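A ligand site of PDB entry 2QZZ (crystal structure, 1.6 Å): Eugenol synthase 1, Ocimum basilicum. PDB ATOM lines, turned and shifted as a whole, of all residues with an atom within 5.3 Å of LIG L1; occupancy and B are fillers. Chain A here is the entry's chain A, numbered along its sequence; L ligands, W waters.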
ATOM      1  N   GLY A  18      31.665  -6.611   9.291  1.00  0.00           N
ATOM      2  CA  GLY A  18      31.653  -6.587  10.744  1.00  0.00           C
ATOM      3  C   GLY A  18      32.409  -7.772  11.323  1.00  0.00           C
ATOM      4  O   GLY A  18      32.204  -8.139  12.487  1.00  0.00           O
ATOM      5  N   THR A  20      35.279  -8.043  12.494  1.00  0.00           N
ATOM      6  CA  THR A  20      36.089  -7.749  13.670  1.00  0.00           C
ATOM      7  C   THR A  20      35.191  -7.567  14.885  1.00  0.00           C
ATOM      8  O   THR A  20      35.668  -7.323  15.986  1.00  0.00           O
ATOM      9  CB  THR A  20      36.892  -6.446  13.500  1.00  0.00           C
ATOM     10  OG1 THR A  20      35.986  -5.343  13.387  1.00  0.00           O
ATOM     11  CG2 THR A  20      37.787  -6.505  12.265  1.00  0.00           C
ATOM     12  N   GLY A  21      33.887  -7.714  14.662  1.00  0.00           N
ATOM     13  CA  GLY A  21      32.924  -7.530  15.737  1.00  0.00           C
ATOM     14  C   GLY A  21      32.876  -8.594  16.825  1.00  0.00           C
ATOM     15  O   GLY A  21      33.566  -9.611  16.763  1.00  0.00           O
ATOM     16  N   TYR A  22      32.038  -8.337  17.824  1.00  0.00           N
ATOM     17  CA  TYR A  22      31.897  -9.253  18.949  1.00  0.00           C
ATOM     18  C   TYR A  22      31.528 -10.661  18.477  1.00  0.00           C
ATOM     19  O   TYR A  22      32.147 -11.631  18.896  1.00  0.00           O
ATOM     20  CB  TYR A  22      30.821  -8.740  19.921  1.00  0.00           C
ATOM     21  CG  TYR A  22      30.691  -9.601  21.152  1.00  0.00           C
ATOM     22  CD1 TYR A  22      31.674  -9.582  22.138  1.00  0.00           C
ATOM     23  CD2 TYR A  22      29.641 -10.505  21.295  1.00  0.00           C
ATOM     24  CE1 TYR A  22      31.605 -10.448  23.243  1.00  0.00           C
ATOM     25  CE2 TYR A  22      29.563 -11.378  22.384  1.00  0.00           C
ATOM     26  CZ  TYR A  22      30.555 -11.344  23.356  1.00  0.00           C
ATOM     27  OH  TYR A  22      30.498 -12.207  24.428  1.00  0.00           O
ATOM     28  N   ILE A  23      30.530 -10.765  17.607  1.00  0.00           N
ATOM     29  CA  ILE A  23      30.134 -12.078  17.106  1.00  0.00           C
ATOM     30  C   ILE A  23      30.796 -12.331  15.754  1.00  0.00           C
ATOM     31  O   ILE A  23      31.074 -13.473  15.386  1.00  0.00           O
ATOM     32  CB  ILE A  23      28.584 -12.211  16.992  1.00  0.00           C
ATOM     33  CG1 ILE A  23      28.180 -13.686  16.869  1.00  0.00           C
ATOM     34  CG2 ILE A  23      28.062 -11.454  15.773  1.00  0.00           C
ATOM     35  CD1 ILE A  23      28.435 -14.508  18.133  1.00  0.00           C
ATOM     36  N   GLY A  24      31.073 -11.250  15.026  1.00  0.00           N
ATOM     37  CA  GLY A  24      31.701 -11.389  13.729  1.00  0.00           C
ATOM     38  C   GLY A  24      33.038 -12.107  13.755  1.00  0.00           C
ATOM     39  O   GLY A  24      33.332 -12.894  12.844  1.00  0.00           O
ATOM     40  N   PHE A  41      35.824  -7.317   5.498  1.00  0.00           N
ATOM     41  CA  PHE A  41      35.717  -5.904   5.168  1.00  0.00           C
ATOM     42  C   PHE A  41      35.839  -5.150   6.485  1.00  0.00           C
ATOM     43  O   PHE A  41      35.164  -5.486   7.456  1.00  0.00           O
ATOM     44  CB  PHE A  41      34.365  -5.613   4.518  1.00  0.00           C
ATOM     45  CG  PHE A  41      34.320  -4.303   3.764  1.00  0.00           C
ATOM     46  CD1 PHE A  41      34.910  -4.190   2.508  1.00  0.00           C
ATOM     47  CD2 PHE A  41      33.685  -3.201   4.312  1.00  0.00           C
ATOM     48  CE1 PHE A  41      34.864  -2.976   1.815  1.00  0.00           C
ATOM     49  CE2 PHE A  41      33.636  -1.987   3.633  1.00  0.00           C
ATOM     50  CZ  PHE A  41      34.227  -1.874   2.377  1.00  0.00           C
ATOM     51  N   THR A  42      36.694  -4.137   6.514  1.00  0.00           N
ATOM     52  CA  THR A  42      36.890  -3.376   7.743  1.00  0.00           C
ATOM     53  C   THR A  42      37.205  -1.915   7.443  1.00  0.00           C
ATOM     54  O   THR A  42      37.777  -1.612   6.400  1.00  0.00           O
ATOM     55  CB  THR A  42      38.040  -4.012   8.573  1.00  0.00           C
ATOM     56  OG1 THR A  42      38.265  -3.250   9.771  1.00  0.00           O
ATOM     57  CG2 THR A  42      39.325  -4.061   7.754  1.00  0.00           C
ATOM     58  N   ARG A  43      36.813  -1.013   8.333  1.00  0.00           N
ATOM     59  CA  ARG A  43      37.066   0.415   8.140  1.00  0.00           C
ATOM     60  C   ARG A  43      38.542   0.736   8.234  1.00  0.00           C
ATOM     61  O   ARG A  43      39.281   0.111   8.996  1.00  0.00           O
ATOM     62  CB  ARG A  43      36.329   1.247   9.191  1.00  0.00           C
ATOM     63  CG  ARG A  43      34.813   1.322   9.018  1.00  0.00           C
ATOM     64  CD  ARG A  43      34.188   1.950  10.239  1.00  0.00           C
ATOM     65  NE  ARG A  43      34.481   1.164  11.437  1.00  0.00           N
ATOM     66  CZ  ARG A  43      34.365   1.611  12.684  1.00  0.00           C
ATOM     67  NH1 ARG A  43      34.647   0.817  13.700  1.00  0.00           N
ATOM     68  NH2 ARG A  43      33.975   2.866  12.900  1.00  0.00           N
ATOM     69  N   SER A  46      39.583   1.549  11.808  1.00  0.00           N
ATOM     70  CA  SER A  46      39.251   0.608  12.873  1.00  0.00           C
ATOM     71  C   SER A  46      40.406   0.446  13.851  1.00  0.00           C
ATOM     72  O   SER A  46      41.571   0.526  13.465  1.00  0.00           O
ATOM     73  CB  SER A  46      38.892  -0.763  12.287  1.00  0.00           C
ATOM     74  OG  SER A  46      38.671  -1.714  13.313  1.00  0.00           O
ATOM     75  N   SER A  47      40.083   0.211  15.126  1.00  0.00           N
ATOM     76  CA  SER A  47      41.101   0.035  16.147  1.00  0.00           C
ATOM     77  C   SER A  47      41.380  -1.446  16.365  1.00  0.00           C
ATOM     78  O   SER A  47      42.177  -1.827  17.228  1.00  0.00           O
ATOM     79  CB  SER A  47      40.642   0.667  17.466  1.00  0.00           C
ATOM     80  OG  SER A  47      39.480   0.023  17.960  1.00  0.00           O
ATOM     81  N   LYS A  48      40.703  -2.284  15.577  1.00  0.00           N
ATOM     82  CA  LYS A  48      40.859  -3.735  15.666  1.00  0.00           C
ATOM     83  C   LYS A  48      42.101  -4.205  14.913  1.00  0.00           C
ATOM     84  O   LYS A  48      42.107  -5.278  14.311  1.00  0.00           O
ATOM     85  CB  LYS A  48      39.623  -4.427  15.067  1.00  0.00           C
ATOM     86  CG  LYS A  48      38.305  -4.027  15.710  1.00  0.00           C
ATOM     87  CD  LYS A  48      38.165  -4.591  17.121  1.00  0.00           C
ATOM     88  CE  LYS A  48      36.808  -4.254  17.717  1.00  0.00           C
ATOM     89  NZ  LYS A  48      35.673  -4.787  16.913  1.00  0.00           N
ATOM     90  N   GLU A  66      35.034   1.696   3.202  1.00  0.00           N
ATOM     91  CA  GLU A  66      33.820   2.188   3.837  1.00  0.00           C
ATOM     92  C   GLU A  66      32.632   1.640   3.061  1.00  0.00           C
ATOM     93  O   GLU A  66      32.744   1.327   1.879  1.00  0.00           O
ATOM     94  CB  GLU A  66      33.783   3.725   3.785  1.00  0.00           C
ATOM     95  CG  GLU A  66      34.916   4.433   4.517  1.00  0.00           C
ATOM     96  CD  GLU A  66      34.815   4.310   6.033  1.00  0.00           C
ATOM     97  OE1 GLU A  66      33.691   4.168   6.564  1.00  0.00           O
ATOM     98  OE2 GLU A  66      35.879   4.366   6.693  1.00  0.00           O
ATOM     99  N   LEU A  67      31.492   1.520   3.732  1.00  0.00           N
ATOM    100  CA  LEU A  67      30.284   1.014   3.101  1.00  0.00           C
ATOM    101  C   LEU A  67      29.799   1.960   2.009  1.00  0.00           C
ATOM    102  O   LEU A  67      29.048   1.553   1.120  1.00  0.00           O
ATOM    103  CB  LEU A  67      29.182   0.838   4.146  1.00  0.00           C
ATOM    104  CG  LEU A  67      29.437  -0.218   5.219  1.00  0.00           C
ATOM    105  CD1 LEU A  67      28.244  -0.286   6.166  1.00  0.00           C
ATOM    106  CD2 LEU A  67      29.672  -1.572   4.572  1.00  0.00           C
ATOM    107  N   ALA A  86      27.523  -8.937   9.985  1.00  0.00           N
ATOM    108  CA  ALA A  86      27.486  -8.986  11.437  1.00  0.00           C
ATOM    109  C   ALA A  86      27.572  -7.565  11.991  1.00  0.00           C
ATOM    110  O   ALA A  86      28.159  -7.324  13.038  1.00  0.00           O
ATOM    111  CB  ALA A  86      28.644  -9.831  11.968  1.00  0.00           C
ATOM    112  N   LEU A  87      26.987  -6.618  11.255  1.00  0.00           N
ATOM    113  CA  LEU A  87      26.999  -5.211  11.683  1.00  0.00           C
ATOM    114  C   LEU A  87      26.129  -4.973  12.929  1.00  0.00           C
ATOM    115  O   LEU A  87      25.247  -5.770  13.245  1.00  0.00           O
ATOM    116  CB  LEU A  87      26.530  -4.309  10.538  1.00  0.00           C
ATOM    117  CG  LEU A  87      27.513  -4.251   9.370  1.00  0.00           C
ATOM    118  CD1 LEU A  87      26.984  -3.305   8.293  1.00  0.00           C
ATOM    119  CD2 LEU A  87      28.876  -3.792   9.863  1.00  0.00           C
ATOM    120  N   ALA A  88      26.400  -3.871  13.611  1.00  0.00           N
ATOM    121  CA  ALA A  88      25.707  -3.490  14.831  1.00  0.00           C
ATOM    122  C   ALA A  88      24.414  -2.740  14.596  1.00  0.00           C
ATOM    123  O   ALA A  88      24.097  -2.290  13.501  1.00  0.00           O
ATOM    124  CB  ALA A  88      26.627  -2.665  15.703  1.00  0.00           C
ATOM    125  N   PHE A  89      23.640  -2.585  15.682  1.00  0.00           N
ATOM    126  CA  PHE A  89      22.364  -1.876  15.674  1.00  0.00           C
ATOM    127  C   PHE A  89      22.390  -0.535  14.938  1.00  0.00           C
ATOM    128  O   PHE A  89      21.524  -0.256  14.118  1.00  0.00           O
ATOM    129  CB  PHE A  89      21.909  -1.619  17.124  1.00  0.00           C
ATOM    130  CG  PHE A  89      21.146  -2.772  17.732  1.00  0.00           C
ATOM    131  CD1 PHE A  89      21.001  -2.870  19.111  1.00  0.00           C
ATOM    132  CD2 PHE A  89      20.516  -3.713  16.927  1.00  0.00           C
ATOM    133  CE1 PHE A  89      20.244  -3.885  19.686  1.00  0.00           C
ATOM    134  CE2 PHE A  89      19.760  -4.728  17.502  1.00  0.00           C
ATOM    135  CZ  PHE A  89      19.628  -4.819  18.868  1.00  0.00           C
ATOM    136  N   GLN A  91      24.053   0.424  12.570  1.00  0.00           N
ATOM    137  CA  GLN A  91      24.266   0.238  11.135  1.00  0.00           C
ATOM    138  C   GLN A  91      23.251  -0.664  10.437  1.00  0.00           C
ATOM    139  O   GLN A  91      23.485  -1.086   9.309  1.00  0.00           O
ATOM    140  CB  GLN A  91      25.669  -0.324  10.915  1.00  0.00           C
ATOM    141  CG  GLN A  91      26.803   0.700  10.968  1.00  0.00           C
ATOM    142  CD  GLN A  91      27.073   1.225  12.368  1.00  0.00           C
ATOM    143  OE1 GLN A  91      27.410   0.461  13.285  1.00  0.00           O
ATOM    144  NE2 GLN A  91      26.935   2.539  12.553  1.00  0.00           N
ATOM    145  N   SER A 114      22.319  -9.099   9.287  1.00  0.00           N
ATOM    146  CA  SER A 114      22.684  -9.075  10.694  1.00  0.00           C
ATOM    147  C   SER A 114      21.516  -9.230  11.656  1.00  0.00           C
ATOM    148  O   SER A 114      21.047  -8.243  12.207  1.00  0.00           O
ATOM    149  CB  SER A 114      23.424  -7.786  11.031  1.00  0.00           C
ATOM    150  OG  SER A 114      24.010  -7.883  12.321  1.00  0.00           O
ATOM    151  N   ASP A 115      21.070 -10.456  11.846  1.00  0.00           N
ATOM    152  CA  ASP A 115      19.990 -10.727  12.783  1.00  0.00           C
ATOM    153  C   ASP A 115      20.694 -11.214  14.037  1.00  0.00           C
ATOM    154  O   ASP A 115      21.020 -10.423  14.927  1.00  0.00           O
ATOM    155  CB  ASP A 115      19.040 -11.784  12.209  1.00  0.00           C
ATOM    156  CG  ASP A 115      18.246 -11.259  11.019  1.00  0.00           C
ATOM    157  OD1 ASP A 115      17.913 -10.060  11.010  1.00  0.00           O
ATOM    158  OD2 ASP A 115      17.941 -12.053  10.103  1.00  0.00           O
ATOM    159  N   PHE A 116      20.950 -12.520  14.094  1.00  0.00           N
ATOM    160  CA  PHE A 116      21.659 -13.174  15.197  1.00  0.00           C
ATOM    161  C   PHE A 116      21.123 -12.911  16.604  1.00  0.00           C
ATOM    162  O   PHE A 116      21.885 -12.676  17.545  1.00  0.00           O
ATOM    163  CB  PHE A 116      23.153 -12.823  15.099  1.00  0.00           C
ATOM    164  CG  PHE A 116      23.770 -13.158  13.764  1.00  0.00           C
ATOM    165  CD1 PHE A 116      24.106 -12.149  12.855  1.00  0.00           C
ATOM    166  CD2 PHE A 116      23.952 -14.484  13.380  1.00  0.00           C
ATOM    167  CE1 PHE A 116      24.614 -12.456  11.588  1.00  0.00           C
ATOM    168  CE2 PHE A 116      24.448 -14.798  12.111  1.00  0.00           C
ATOM    169  CZ  PHE A 116      24.782 -13.788  11.216  1.00  0.00           C
ATOM    170  N   GLY A 117      19.803 -12.994  16.757  1.00  0.00           N
ATOM    171  CA  GLY A 117      19.194 -12.775  18.053  1.00  0.00           C
ATOM    172  C   GLY A 117      17.791 -13.374  18.076  1.00  0.00           C
ATOM    173  O   GLY A 117      17.609 -14.558  17.798  1.00  0.00           O
ATOM    174  N   LYS A 136      15.390  -4.371  11.019  1.00  0.00           N
ATOM    175  CA  LYS A 136      15.925  -5.646  10.554  1.00  0.00           C
ATOM    176  C   LYS A 136      14.904  -6.315   9.631  1.00  0.00           C
ATOM    177  O   LYS A 136      15.277  -6.984   8.664  1.00  0.00           O
ATOM    178  CB  LYS A 136      16.268  -6.543  11.750  1.00  0.00           C
ATOM    179  CG  LYS A 136      17.437  -6.013  12.560  1.00  0.00           C
ATOM    180  CD  LYS A 136      17.953  -7.051  13.524  1.00  0.00           C
ATOM    181  CE  LYS A 136      19.186  -6.553  14.245  1.00  0.00           C
ATOM    182  NZ  LYS A 136      19.781  -7.592  15.122  1.00  0.00           N
ATOM    183  N   ASN A 156      19.462 -16.612  19.151  1.00  0.00           N
ATOM    184  CA  ASN A 156      18.985 -16.482  20.523  1.00  0.00           C
ATOM    185  C   ASN A 156      20.044 -15.732  21.371  1.00  0.00           C
ATOM    186  O   ASN A 156      20.795 -14.937  20.818  1.00  0.00           O
ATOM    187  CB  ASN A 156      18.609 -17.849  21.096  1.00  0.00           C
ATOM    188  CG  ASN A 156      17.249 -18.321  20.582  1.00  0.00           C
ATOM    189  OD1 ASN A 156      16.326 -17.521  20.450  1.00  0.00           O
ATOM    190  ND2 ASN A 156      17.133 -19.617  20.306  1.00  0.00           N
ATOM    191  N   CYS A 157      20.114 -15.982  22.676  1.00  0.00           N
ATOM    192  CA  CYS A 157      21.076 -15.231  23.507  1.00  0.00           C
ATOM    193  C   CYS A 157      22.559 -15.605  23.400  1.00  0.00           C
ATOM    194  O   CYS A 157      22.909 -16.776  23.460  1.00  0.00           O
ATOM    195  CB  CYS A 157      20.666 -15.314  24.992  1.00  0.00           C
ATOM    196  SG  CYS A 157      19.005 -14.691  25.383  1.00  0.00           S
ATOM    197  N   PHE A 158      23.424 -14.598  23.259  1.00  0.00           N
ATOM    198  CA  PHE A 158      24.866 -14.872  23.205  1.00  0.00           C
ATOM    199  C   PHE A 158      25.169 -15.259  24.661  1.00  0.00           C
ATOM    200  O   PHE A 158      25.004 -14.455  25.585  1.00  0.00           O
ATOM    201  CB  PHE A 158      25.652 -13.610  22.797  1.00  0.00           C
ATOM    202  CG  PHE A 158      25.565 -13.263  21.328  1.00  0.00           C
ATOM    203  CD1 PHE A 158      24.744 -13.975  20.453  1.00  0.00           C
ATOM    204  CD2 PHE A 158      26.278 -12.181  20.836  1.00  0.00           C
ATOM    205  CE1 PHE A 158      24.645 -13.596  19.103  1.00  0.00           C
ATOM    206  CE2 PHE A 158      26.180 -11.802  19.486  1.00  0.00           C
ATOM    207  CZ  PHE A 158      25.356 -12.513  18.625  1.00  0.00           C
ATOM    208  N   TYR A 161      28.062 -13.435  26.772  1.00  0.00           N
ATOM    209  CA  TYR A 161      27.578 -12.090  26.941  1.00  0.00           C
ATOM    210  C   TYR A 161      26.597 -12.066  28.106  1.00  0.00           C
ATOM    211  O   TYR A 161      26.754 -11.295  29.048  1.00  0.00           O
ATOM    212  CB  TYR A 161      26.883 -11.626  25.654  1.00  0.00           C
ATOM    213  CG  TYR A 161      26.477 -10.157  25.623  1.00  0.00           C
ATOM    214  CD1 TYR A 161      27.143  -9.250  24.801  1.00  0.00           C
ATOM    215  CD2 TYR A 161      25.398  -9.699  26.382  1.00  0.00           C
ATOM    216  CE1 TYR A 161      26.743  -7.923  24.733  1.00  0.00           C
ATOM    217  CE2 TYR A 161      24.991  -8.362  26.327  1.00  0.00           C
ATOM    218  CZ  TYR A 161      25.673  -7.482  25.494  1.00  0.00           C
ATOM    219  OH  TYR A 161      25.288  -6.168  25.437  1.00  0.00           O
ATOM    220  N   PHE A 162      25.583 -12.941  28.045  1.00  0.00           N
ATOM    221  CA  PHE A 162      24.575 -12.937  29.084  1.00  0.00           C
ATOM    222  C   PHE A 162      24.881 -13.619  30.401  1.00  0.00           C
ATOM    223  O   PHE A 162      24.239 -13.318  31.410  1.00  0.00           O
ATOM    224  CB  PHE A 162      23.246 -13.410  28.525  1.00  0.00           C
ATOM    225  CG  PHE A 162      22.533 -12.328  27.778  1.00  0.00           C
ATOM    226  CD1 PHE A 162      22.589 -12.272  26.387  1.00  0.00           C
ATOM    227  CD2 PHE A 162      21.914 -11.303  28.468  1.00  0.00           C
ATOM    228  CE1 PHE A 162      22.024 -11.190  25.699  1.00  0.00           C
ATOM    229  CE2 PHE A 162      21.355 -10.217  27.789  1.00  0.00           C
ATOM    230  CZ  PHE A 162      21.414 -10.157  26.419  1.00  0.00           C
ATOM    231  N   ALA A 316      26.955  -4.348  23.962  1.00  0.00           N
ATOM    232  CA  ALA A 316      26.614  -4.029  22.588  1.00  0.00           C
ATOM    233  C   ALA A 316      26.532  -2.517  22.372  1.00  0.00           C
ATOM    234  O   ALA A 316      26.439  -1.748  23.331  1.00  0.00           O
ATOM    235  CB  ALA A 316      25.278  -4.677  22.222  1.00  0.00           C
ATOM    236  N   ALA A 317      26.584  -2.109  21.117  1.00  0.00           N
ATOM    237  CA  ALA A 317      26.509  -0.691  20.777  1.00  0.00           C
ATOM    238  C   ALA A 317      25.072  -0.316  20.433  1.00  0.00           C
ATOM    239  O   ALA A 317      24.391  -1.066  19.719  1.00  0.00           O
ATOM    240  CB  ALA A 317      27.422  -0.373  19.602  1.00  0.00           C
HETATM  241  P1  LIG L   1      29.871  -4.930  17.092  1.00  0.00           P
HETATM  242  O1  LIG L   1      29.411  -3.785  17.918  1.00  0.00           O
HETATM  243  O2  LIG L   1      30.973  -5.792  17.564  1.00  0.00           O
HETATM  244  O3  LIG L   1      30.159  -4.298  15.644  1.00  0.00           O
HETATM  245  C1  LIG L   1      30.522  -5.141  14.539  1.00  0.00           C
HETATM  246  C2  LIG L   1      31.420  -4.319  13.650  1.00  0.00           C
HETATM  247  O4  LIG L   1      30.845  -3.092  12.963  1.00  0.00           O
HETATM  248  C3  LIG L   1      32.605  -3.586  14.261  1.00  0.00           C
HETATM  249  O5  LIG L   1      33.599  -4.505  14.676  1.00  0.00           O
HETATM  250  C4  LIG L   1      33.099  -2.599  13.199  1.00  0.00           C
HETATM  251  O6  LIG L   1      34.085  -3.202  12.367  1.00  0.00           O
HETATM  252  C5  LIG L   1      31.852  -2.281  12.394  1.00  0.00           C
HETATM  253  N1  LIG L   1      31.413  -0.879  12.533  1.00  0.00           N
HETATM  254  C6  LIG L   1      31.265  -0.169  13.721  1.00  0.00           C
HETATM  255  N2  LIG L   1      30.857   1.071  13.548  1.00  0.00           N
HETATM  256  C7  LIG L   1      30.729   1.177  12.196  1.00  0.00           C
HETATM  257  C8  LIG L   1      30.336   2.256  11.365  1.00  0.00           C
HETATM  258  N3  LIG L   1      29.991   3.449  11.879  1.00  0.00           N
HETATM  259  N4  LIG L   1      30.314   2.042  10.015  1.00  0.00           N
HETATM  260  C9  LIG L   1      30.664   0.828   9.496  1.00  0.00           C
HETATM  261  N5  LIG L   1      31.066  -0.263  10.200  1.00  0.00           N
HETATM  262  C10 LIG L   1      31.068  -0.014  11.546  1.00  0.00           C
HETATM  263  O7  LIG L   1      28.544  -5.804  16.728  1.00  0.00           O
HETATM  264  P2  LIG L   1      27.930  -6.997  17.621  1.00  0.00           P
HETATM  265  O8  LIG L   1      27.847  -6.623  19.048  1.00  0.00           O
HETATM  266  O9  LIG L   1      28.713  -8.205  17.287  1.00  0.00           O
HETATM  267  O10 LIG L   1      26.468  -7.216  17.009  1.00  0.00           O
HETATM  268  C11 LIG L   1      26.277  -7.832  15.718  1.00  0.00           C
HETATM  269  C12 LIG L   1      24.888  -8.427  15.628  1.00  0.00           C
HETATM  270  O11 LIG L   1      24.701  -9.310  16.765  1.00  0.00           O
HETATM  271  C13 LIG L   1      23.755  -7.371  15.616  1.00  0.00           C
HETATM  272  O12 LIG L   1      22.744  -7.722  14.696  1.00  0.00           O
HETATM  273  C14 LIG L   1      23.345  -7.401  17.063  1.00  0.00           C
HETATM  274  O13 LIG L   1      22.017  -6.934  17.206  1.00  0.00           O
HETATM  275  C15 LIG L   1      23.538  -8.837  17.466  1.00  0.00           C
HETATM  276  N6  LIG L   1      23.670  -9.006  18.936  1.00  0.00           N
HETATM  277  C16 LIG L   1      22.943 -10.041  19.502  1.00  0.00           C
HETATM  278  C17 LIG L   1      23.220 -10.462  20.812  1.00  0.00           C
HETATM  279  C18 LIG L   1      22.509 -11.645  21.415  1.00  0.00           C
HETATM  280  O14 LIG L   1      22.615 -11.876  22.625  1.00  0.00           O
HETATM  281  N7  LIG L   1      21.785 -12.422  20.588  1.00  0.00           N
HETATM  282  C19 LIG L   1      24.218  -9.770  21.573  1.00  0.00           C
HETATM  283  C20 LIG L   1      24.947  -8.716  20.970  1.00  0.00           C
HETATM  284  C21 LIG L   1      24.689  -8.354  19.651  1.00  0.00           C
HETATM  285  P3  LIG L   1      35.419  -2.452  11.854  1.00  0.00           P
HETATM  286  O15 LIG L   1      36.022  -1.709  13.028  1.00  0.00           O
HETATM  287  O16 LIG L   1      36.214  -3.621  11.327  1.00  0.00           O
HETATM  288  O17 LIG L   1      34.984  -1.516  10.735  1.00  0.00           O
HETATM  289  O1  LG2 L   2      20.678  -4.827  25.215  1.00  0.00           O
HETATM  290  C1  LG2 L   2      21.204  -5.907  24.942  1.00  0.00           C
HETATM  291  O2  LG2 L   2      21.826  -6.686  26.007  1.00  0.00           O
HETATM  292  C2  LG2 L   2      21.721  -6.319  27.388  1.00  0.00           C
HETATM  293  C3  LG2 L   2      20.308  -6.550  27.875  1.00  0.00           C
HETATM  294  C4  LG2 L   2      21.198  -6.400  23.526  1.00  0.00           C
HETATM  295  C5  LG2 L   2      22.535  -6.914  22.992  1.00  0.00           C
HETATM  296  C6  LG2 L   2      21.400  -7.907  23.346  1.00  0.00           C
HETATM  297  C7  LG2 L   2      20.543  -8.441  22.215  1.00  0.00           C
HETATM  298  C8  LG2 L   2      19.833  -9.679  22.398  1.00  0.00           C
HETATM  299  C9  LG2 L   2      19.004 -10.210  21.350  1.00  0.00           C
HETATM  300  O3  LG2 L   2      18.302 -11.393  21.474  1.00  0.00           O
HETATM  301  C10 LG2 L   2      18.818 -12.535  22.170  1.00  0.00           C
HETATM  302  C11 LG2 L   2      20.415  -7.729  20.976  1.00  0.00           C
HETATM  303  C12 LG2 L   2      19.600  -8.228  19.929  1.00  0.00           C
HETATM  304  C13 LG2 L   2      18.887  -9.438  20.074  1.00  0.00           C
HETATM  305  O4  LG2 L   2      18.096  -9.918  19.067  1.00  0.00           O
HETATM  306  O   HOH W   1      28.290  -1.973  12.636  1.00  0.00           O
HETATM  307  O   HOH W   2      30.669  -3.260  20.399  1.00  0.00           O
HETATM  308  O   HOH W   3      30.021  -8.472  14.989  1.00  0.00           O
HETATM  309  O   HOH W   4      34.945  -5.837  10.295  1.00  0.00           O
HETATM  310  O   HOH W   5      35.554  -2.214  15.689  1.00  0.00           O
HETATM  311  O   HOH W   6      28.154  -7.240  21.726  1.00  0.00           O
HETATM  312  O   HOH W   7      33.276  -4.928  18.727  1.00  0.00           O
HETATM  313  O   HOH W   8      27.139  -3.992  19.302  1.00  0.00           O
HETATM  314  O   HOH W   9      31.938   1.922   6.679  1.00  0.00           O
HETATM  315  O   HOH W  10      33.001  -1.960   8.834  1.00  0.00           O
HETATM  316  O   HOH W  11      30.076  -1.138  16.934  1.00  0.00           O
HETATM  317  O   HOH W  12      22.878  -5.494  19.565  1.00  0.00           O
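Water W3 lies within hydrogen-bond range of an oxygen (O9) of LIG L1, the backbone carbonyl oxygen (O) of Ala 86, the backbone NH (N) of Gly 24, the backbone carbonyl oxygen (O) of Gly 18 and the backbone NH (N) of Tyr 22.
Water W8 lies within hydrogen-bond range of O1 of LIG L1 (2.7 Å) and N of Ala 317 (2.7 Å).
Water W7 lies within hydrogen-bond range of O2 of LIG L1 (2.7 Å) and NZ of Lys 48 (3.0 Å).
Water W5 bridges an oxygen (O15) of LIG L1 (2.7 Å) and the side-chain amino group of Lys 48 (2.9 Å).
Water W4 lies within hydrogen-bond range of O16 of LIG L1, O of Phe 41 and N of Thr 20.
Water W9 bridges OE1 of Glu 66 (2.9 Å) and N of Leu 67 (3.0 Å).
The side-chain hydroxyl (OG) of Ser 46 lies within hydrogen-bond range of the backbone NH (N) of Lys 48.
The backbone carbonyl oxygen of Thr 20 sits at hydrogen-bond distance from the side-chain amino group of Lys 48 (2.7 Å).
NZ of Lys 136 sits close to O of Ser 114, 3.2 Å away.
The backbone carbonyl oxygen (O) of Leu 87 lies within hydrogen-bond range of the side-chain hydroxyl (OG) of Ser 114, at 2.6 Å.
The backbone carbonyl oxygen of Gly 117 lies within hydrogen-bond range of the backbone NH of Asn 156 (3.1 Å).
The side-chain amino group (NZ) of Lys 136 is in hydrogen-bond range of the backbone carbonyl oxygen (O) of Asp 115, at 3.1 Å.
The side-chain hydroxyl (OG1) of Thr 42 lies within hydrogen-bond range of an oxygen (O16) of LIG L1.
An oxygen (O15) of LIG L1 sits at hydrogen-bond distance from the side-chain hydroxyl (OG) of Ser 46 (2.7 Å).
The side-chain hydroxyl (OG1) of Thr 20 is in hydrogen-bond range of an oxygen (O16) of LIG L1, at 2.7 Å.
O12 of LIG L1 lies within hydrogen-bond range of O of Ser 114 (3.1 Å).
OG of Ser 114 is in hydrogen-bond range of O12 of LIG L1.
O of Asn 156 is in hydrogen-bond range of N7 of LIG L1 (2.7 Å).
The backbone NH of Tyr 22 sits at hydrogen-bond distance from an oxygen (O2) of LIG L1 (2.8 Å).
N of Arg 43 is in hydrogen-bond range of O17 of LIG L1 (3.1 Å).
O17 of LIG L1 is in salt-bridge range of NE of Arg 43, at 2.8 Å.
An oxygen (O14) of LIG L1 sits at hydrogen-bond distance from the backbone NH of Phe 158 (2.9 Å).
O12 of LIG L1 lies within hydrogen-bond range of NZ of Lys 136 (3.0 Å).
O of Phe 116 is in hydrogen-bond range of N7 of LIG L1 (3.1 Å).
The side-chain amino group (NZ) of Lys 48 sits at hydrogen-bond distance from an oxygen (O5) of LIG L1 (3.1 Å).
The backbone NH (N) of Ile 23 is in hydrogen-bond range of an oxygen (O9) of LIG L1, at 3.2 Å.
N of Gly 21 is in hydrogen-bond range of O5 of LIG L1, at 3.2 Å.
The backbone carbonyl oxygen (O) of Asp 115 sits at hydrogen-bond distance from an oxygen (O12) of LIG L1 (3.2 Å).
O12 of LIG L1 sits close to O of Leu 87 (3.5 Å).
A nitrogen (N3) of LIG L1 sits close to the side-chain amide nitrogen (NE2) of Gln 91.
Merely in contact with LIG L1: Phe 89 (3.2 Å), Phe 162 (3.2 Å), Ala 86 (3.3 Å), Gly 117 (3.6 Å), Gly 18 (3.7 Å), Ala 88 (3.7 Å) and Cys 157 (3.8 Å).
Within 4 Å of LIG L1: Gly 18, Thr 20, Gly 21, Tyr 22, Ile 23, Thr 42, Arg 43, Ser 46, Lys 48, Ala 86, Leu 87, Ala 88, Phe 89, Gln 91, Ser 114, Asp 115, Phe 116, Gly 117, Lys 136, Asn 156, Cys 157, Phe 158 and Phe 162.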
